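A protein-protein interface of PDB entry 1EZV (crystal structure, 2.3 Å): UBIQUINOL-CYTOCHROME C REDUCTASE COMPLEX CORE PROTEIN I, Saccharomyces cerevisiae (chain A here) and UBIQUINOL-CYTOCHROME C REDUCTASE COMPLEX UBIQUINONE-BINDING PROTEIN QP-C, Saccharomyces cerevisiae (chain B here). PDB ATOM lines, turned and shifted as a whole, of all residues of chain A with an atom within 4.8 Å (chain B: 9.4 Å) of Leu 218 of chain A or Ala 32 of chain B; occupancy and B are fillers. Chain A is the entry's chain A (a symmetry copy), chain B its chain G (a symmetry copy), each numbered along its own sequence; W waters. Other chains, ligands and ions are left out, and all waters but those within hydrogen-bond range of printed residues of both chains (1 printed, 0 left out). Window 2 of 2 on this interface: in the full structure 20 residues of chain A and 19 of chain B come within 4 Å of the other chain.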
ATOM      1  N   THR A 140     -25.717 -30.908   4.090  1.00  0.00           N
ATOM      2  CA  THR A 140     -25.315 -29.646   3.471  1.00  0.00           C
ATOM      3  C   THR A 140     -25.075 -28.544   4.490  1.00  0.00           C
ATOM      4  O   THR A 140     -24.113 -27.786   4.365  1.00  0.00           O
ATOM      5  CB  THR A 140     -26.329 -29.162   2.394  1.00  0.00           C
ATOM      6  OG1 THR A 140     -25.773 -28.040   1.692  1.00  0.00           O
ATOM      7  CG2 THR A 140     -27.665 -28.757   3.018  1.00  0.00           C
ATOM      8  N   ALA A 141     -25.875 -28.527   5.554  1.00  0.00           N
ATOM      9  CA  ALA A 141     -25.747 -27.509   6.593  1.00  0.00           C
ATOM     10  C   ALA A 141     -24.372 -27.559   7.245  1.00  0.00           C
ATOM     11  O   ALA A 141     -23.773 -26.518   7.530  1.00  0.00           O
ATOM     12  CB  ALA A 141     -26.826 -27.695   7.644  1.00  0.00           C
ATOM     13  N   GLN A 143     -21.573 -29.357   5.962  1.00  0.00           N
ATOM     14  CA  GLN A 143     -20.684 -30.008   4.999  1.00  0.00           C
ATOM     15  C   GLN A 143     -19.200 -29.917   5.360  1.00  0.00           C
ATOM     16  O   GLN A 143     -18.749 -28.911   5.921  1.00  0.00           O
ATOM     17  CB  GLN A 143     -20.918 -29.439   3.597  1.00  0.00           C
ATOM     18  CG  GLN A 143     -20.650 -27.949   3.452  1.00  0.00           C
ATOM     19  CD  GLN A 143     -21.130 -27.400   2.115  1.00  0.00           C
ATOM     20  OE1 GLN A 143     -22.328 -27.212   1.902  1.00  0.00           O
ATOM     21  NE2 GLN A 143     -20.196 -27.132   1.214  1.00  0.00           N
ATOM     22  N   ALA A 216     -19.216 -26.723  11.931  1.00  0.00           N
ATOM     23  CA  ALA A 216     -19.618 -25.380  11.526  1.00  0.00           C
ATOM     24  C   ALA A 216     -20.791 -25.389  10.548  1.00  0.00           C
ATOM     25  O   ALA A 216     -20.896 -26.261   9.679  1.00  0.00           O
ATOM     26  CB  ALA A 216     -18.438 -24.641  10.918  1.00  0.00           C
ATOM     27  N   PHE A 217     -21.698 -24.434  10.739  1.00  0.00           N
ATOM     28  CA  PHE A 217     -22.853 -24.257   9.863  1.00  0.00           C
ATOM     29  C   PHE A 217     -22.446 -23.460   8.625  1.00  0.00           C
ATOM     30  O   PHE A 217     -21.755 -22.442   8.719  1.00  0.00           O
ATOM     31  CB  PHE A 217     -23.976 -23.530  10.617  1.00  0.00           C
ATOM     32  CG  PHE A 217     -25.245 -23.369   9.826  1.00  0.00           C
ATOM     33  CD1 PHE A 217     -26.234 -24.346   9.870  1.00  0.00           C
ATOM     34  CD2 PHE A 217     -25.465 -22.223   9.066  1.00  0.00           C
ATOM     35  CE1 PHE A 217     -27.425 -24.182   9.170  1.00  0.00           C
ATOM     36  CE2 PHE A 217     -26.648 -22.047   8.363  1.00  0.00           C
ATOM     37  CZ  PHE A 217     -27.630 -23.026   8.413  1.00  0.00           C
ATOM     38  N   LEU A 218     -22.806 -23.978   7.460  1.00  0.00           N
ATOM     39  CA  LEU A 218     -22.616 -23.245   6.218  1.00  0.00           C
ATOM     40  C   LEU A 218     -23.953 -23.110   5.492  1.00  0.00           C
ATOM     41  O   LEU A 218     -24.600 -24.113   5.172  1.00  0.00           O
ATOM     42  CB  LEU A 218     -21.608 -23.967   5.326  1.00  0.00           C
ATOM     43  CG  LEU A 218     -21.277 -23.235   4.029  1.00  0.00           C
ATOM     44  CD1 LEU A 218     -20.372 -22.047   4.327  1.00  0.00           C
ATOM     45  CD2 LEU A 218     -20.618 -24.193   3.066  1.00  0.00           C
ATOM     46  N   GLY A 219     -24.375 -21.866   5.273  1.00  0.00           N
ATOM     47  CA  GLY A 219     -25.618 -21.600   4.561  1.00  0.00           C
ATOM     48  C   GLY A 219     -25.557 -22.093   3.129  1.00  0.00           C
ATOM     49  O   GLY A 219     -24.686 -21.679   2.375  1.00  0.00           O
ATOM     50  N   SER A 220     -26.466 -22.995   2.767  1.00  0.00           N
ATOM     51  CA  SER A 220     -26.356 -23.735   1.520  1.00  0.00           C
ATOM     52  C   SER A 220     -27.601 -24.574   1.277  1.00  0.00           C
ATOM     53  O   SER A 220     -28.490 -24.623   2.110  1.00  0.00           O
ATOM     54  CB  SER A 220     -25.127 -24.644   1.570  1.00  0.00           C
ATOM     55  OG  SER A 220     -25.232 -25.565   2.637  1.00  0.00           O
ATOM     56  N   ASP A 403     -28.184 -16.710   7.440  1.00  0.00           N
ATOM     57  CA  ASP A 403     -28.125 -17.741   6.419  1.00  0.00           C
ATOM     58  C   ASP A 403     -29.006 -18.913   6.789  1.00  0.00           C
ATOM     59  O   ASP A 403     -29.277 -19.147   7.959  1.00  0.00           O
ATOM     60  CB  ASP A 403     -26.684 -18.222   6.236  1.00  0.00           C
ATOM     61  CG  ASP A 403     -25.916 -17.402   5.221  1.00  0.00           C
ATOM     62  OD1 ASP A 403     -24.666 -17.503   5.188  1.00  0.00           O
ATOM     63  OD2 ASP A 403     -26.562 -16.698   4.416  1.00  0.00           O
ATOM     64  N   ALA A 405     -30.202 -23.180   5.569  1.00  0.00           N
ATOM     65  CA  ALA A 405     -29.807 -24.379   4.869  1.00  0.00           C
ATOM     66  C   ALA A 405     -31.078 -25.062   4.416  1.00  0.00           C
ATOM     67  O   ALA A 405     -32.079 -25.059   5.141  1.00  0.00           O
ATOM     68  CB  ALA A 405     -29.013 -25.279   5.793  1.00  0.00           C
ATOM     69  N   ALA B  27     -25.684 -25.644  -3.866  1.00  0.00           N
ATOM     70  CA  ALA B  27     -25.257 -24.255  -3.910  1.00  0.00           C
ATOM     71  C   ALA B  27     -24.920 -23.745  -2.512  1.00  0.00           C
ATOM     72  O   ALA B  27     -25.306 -24.349  -1.514  1.00  0.00           O
ATOM     73  CB  ALA B  27     -26.353 -23.382  -4.553  1.00  0.00           C
ATOM     74  N   VAL B  28     -24.301 -22.571  -2.456  1.00  0.00           N
ATOM     75  CA  VAL B  28     -23.830 -22.003  -1.205  1.00  0.00           C
ATOM     76  C   VAL B  28     -24.177 -20.516  -1.166  1.00  0.00           C
ATOM     77  O   VAL B  28     -23.973 -19.799  -2.150  1.00  0.00           O
ATOM     78  CB  VAL B  28     -22.287 -22.180  -1.064  1.00  0.00           C
ATOM     79  CG1 VAL B  28     -21.752 -21.306   0.063  1.00  0.00           C
ATOM     80  CG2 VAL B  28     -21.954 -23.644  -0.784  1.00  0.00           C
ATOM     81  N   SER B  29     -24.656 -20.053  -0.014  1.00  0.00           N
ATOM     82  CA  SER B  29     -25.066 -18.666   0.153  1.00  0.00           C
ATOM     83  C   SER B  29     -23.986 -17.698  -0.325  1.00  0.00           C
ATOM     84  O   SER B  29     -22.796 -17.895  -0.054  1.00  0.00           O
ATOM     85  CB  SER B  29     -25.397 -18.376   1.618  1.00  0.00           C
ATOM     86  OG  SER B  29     -25.658 -16.995   1.825  1.00  0.00           O
ATOM     87  N   PRO B  30     -24.388 -16.677  -1.104  1.00  0.00           N
ATOM     88  CA  PRO B  30     -23.532 -15.535  -1.433  1.00  0.00           C
ATOM     89  C   PRO B  30     -22.908 -14.917  -0.194  1.00  0.00           C
ATOM     90  O   PRO B  30     -21.797 -14.400  -0.249  1.00  0.00           O
ATOM     91  CB  PRO B  30     -24.489 -14.566  -2.124  1.00  0.00           C
ATOM     92  CG  PRO B  30     -25.477 -15.471  -2.783  1.00  0.00           C
ATOM     93  CD  PRO B  30     -25.686 -16.599  -1.801  1.00  0.00           C
ATOM     94  N   TYR B  31     -23.624 -14.979   0.924  1.00  0.00           N
ATOM     95  CA  TYR B  31     -23.136 -14.407   2.173  1.00  0.00           C
ATOM     96  C   TYR B  31     -21.896 -15.137   2.687  1.00  0.00           C
ATOM     97  O   TYR B  31     -20.958 -14.503   3.175  1.00  0.00           O
ATOM     98  CB  TYR B  31     -24.233 -14.441   3.236  1.00  0.00           C
ATOM     99  CG  TYR B  31     -25.281 -13.374   3.058  1.00  0.00           C
ATOM    100  CD1 TYR B  31     -26.466 -13.641   2.365  1.00  0.00           C
ATOM    101  CD2 TYR B  31     -25.119 -12.113   3.632  1.00  0.00           C
ATOM    102  CE1 TYR B  31     -27.470 -12.684   2.265  1.00  0.00           C
ATOM    103  CE2 TYR B  31     -26.115 -11.142   3.528  1.00  0.00           C
ATOM    104  CZ  TYR B  31     -27.290 -11.436   2.854  1.00  0.00           C
ATOM    105  OH  TYR B  31     -28.313 -10.508   2.825  1.00  0.00           O
ATOM    106  N   ALA B  32     -21.844 -16.443   2.431  1.00  0.00           N
ATOM    107  CA  ALA B  32     -20.757 -17.297   2.899  1.00  0.00           C
ATOM    108  C   ALA B  32     -19.569 -17.310   1.942  1.00  0.00           C
ATOM    109  O   ALA B  32     -18.567 -17.977   2.200  1.00  0.00           O
ATOM    110  CB  ALA B  32     -21.270 -18.718   3.106  1.00  0.00           C
ATOM    111  N   GLN B  33     -19.698 -16.611   0.819  1.00  0.00           N
ATOM    112  CA  GLN B  33     -18.683 -16.659  -0.225  1.00  0.00           C
ATOM    113  C   GLN B  33     -17.734 -15.482  -0.135  1.00  0.00           C
ATOM    114  O   GLN B  33     -18.056 -14.448   0.452  1.00  0.00           O
ATOM    115  CB  GLN B  33     -19.329 -16.692  -1.611  1.00  0.00           C
ATOM    116  CG  GLN B  33     -20.155 -17.936  -1.881  1.00  0.00           C
ATOM    117  CD  GLN B  33     -20.662 -18.007  -3.308  1.00  0.00           C
ATOM    118  OE1 GLN B  33     -19.998 -17.546  -4.238  1.00  0.00           O
ATOM    119  NE2 GLN B  33     -21.838 -18.599  -3.492  1.00  0.00           N
ATOM    120  N   LYS B  34     -16.555 -15.660  -0.718  1.00  0.00           N
ATOM    121  CA  LYS B  34     -15.512 -14.647  -0.707  1.00  0.00           C
ATOM    122  C   LYS B  34     -16.030 -13.352  -1.319  1.00  0.00           C
ATOM    123  O   LYS B  34     -16.489 -13.342  -2.464  1.00  0.00           O
ATOM    124  CB  LYS B  34     -14.302 -15.153  -1.496  1.00  0.00           C
ATOM    125  CG  LYS B  34     -12.959 -14.606  -1.034  1.00  0.00           C
ATOM    126  CD  LYS B  34     -11.930 -15.726  -0.897  1.00  0.00           C
ATOM    127  CE  LYS B  34     -11.787 -16.524  -2.194  1.00  0.00           C
ATOM    128  NZ  LYS B  34     -11.410 -17.948  -1.949  1.00  0.00           N
ATOM    129  N   PRO B  35     -16.012 -12.254  -0.542  1.00  0.00           N
ATOM    130  CA  PRO B  35     -16.165 -10.895  -1.074  1.00  0.00           C
ATOM    131  C   PRO B  35     -15.382 -10.714  -2.368  1.00  0.00           C
ATOM    132  O   PRO B  35     -14.305 -11.288  -2.538  1.00  0.00           O
ATOM    133  CB  PRO B  35     -15.628  -9.999   0.049  1.00  0.00           C
ATOM    134  CG  PRO B  35     -14.964 -10.938   1.037  1.00  0.00           C
ATOM    135  CD  PRO B  35     -15.699 -12.229   0.894  1.00  0.00           C
HETATM  136  O   HOH W   1     -24.176 -27.314  -0.891  1.00  0.00           O
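Among the printed residues, pairs that only touch across the chains: Leu 218 of chain A with Ala 32 of chain B (3.7 Å), Gly 219 of chain A with Val 28 of chain B (3.7 Å), Ser 220 of chain A with Ala 27 of chain B (3.1 Å) and Asp 403 of chain A with Tyr 31 of chain B (3.5 Å).
Of the 10 printed residues of chain A, 4 touch a printed residue of chain B.
Among the printed residues, no Asp or Glu carboxylate lies within 4 Å of a Lys or Arg side-chain nitrogen of the other chain.
Of chain A, only Leu 218 comes within 4 Å of Ala 32 of chain B.
Ala 141 of chain A touches none of the printed residues of chain B.
Of chain B, only Val 28 (3.7 Å) and Ser 29 (2.9 Å) come within 4 Å of Gly 219 of chain A.
Printed residues of chain B within 4 Å of Asp 403 of chain A: Ser 29 (2.8 Å) and Tyr 31 (3.5 Å).
Of the printed residues of chain A, Val 28 of chain B touches Gly 219.
Of the printed residues of chain A, Ser 29 of chain B touches Gly 219 and Asp 403.
Pro 35 of chain B touches none of the printed residues of chain A.
The nearest printed residue of chain A that does not touch Ala 27 of chain B is Gly 219 of chain A (4.8 Å).
Water W1 lies within hydrogen-bond range of OG1 of Thr 140 of chain A (3.1 Å), O of Ala 27 of chain B (3.2 Å) and OE1 of Gln 143 of chain A (3.4 Å).
O of Gly 219 of chain A sits at hydrogen-bond distance from N of Ser 29 of chain B (2.9 Å).
The side-chain carboxylate (OD2) of Asp 403 of chain A sits at hydrogen-bond distance from the side-chain hydroxyl (OG) of Ser 29 of chain B (2.8 Å).
O of Leu 218 of chain A lies within hydrogen-bond range of OG of Ser 220 of chain A.
OE1 of Gln 143 of chain A is in hydrogen-bond range of OG of Ser 220 of chain A (3.4 Å).
The side-chain hydroxyl (OG) of Ser 29 of chain B sits at hydrogen-bond distance from the backbone NH (N) of Tyr 31 of chain B (3.0 Å).
The side-chain amide nitrogen (NE2) of Gln 33 of chain B is in hydrogen-bond range of the backbone carbonyl oxygen (O) of Val 28 of chain B (2.8 Å).
O of Ala 141 of chain A lies within hydrogen-bond range of N of Leu 218 of chain A (2.7 Å).
The side-chain hydroxyl (OG1) of Thr 140 of chain A sits at hydrogen-bond distance from the side-chain hydroxyl (OG) of Ser 220 of chain A (2.7 Å).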
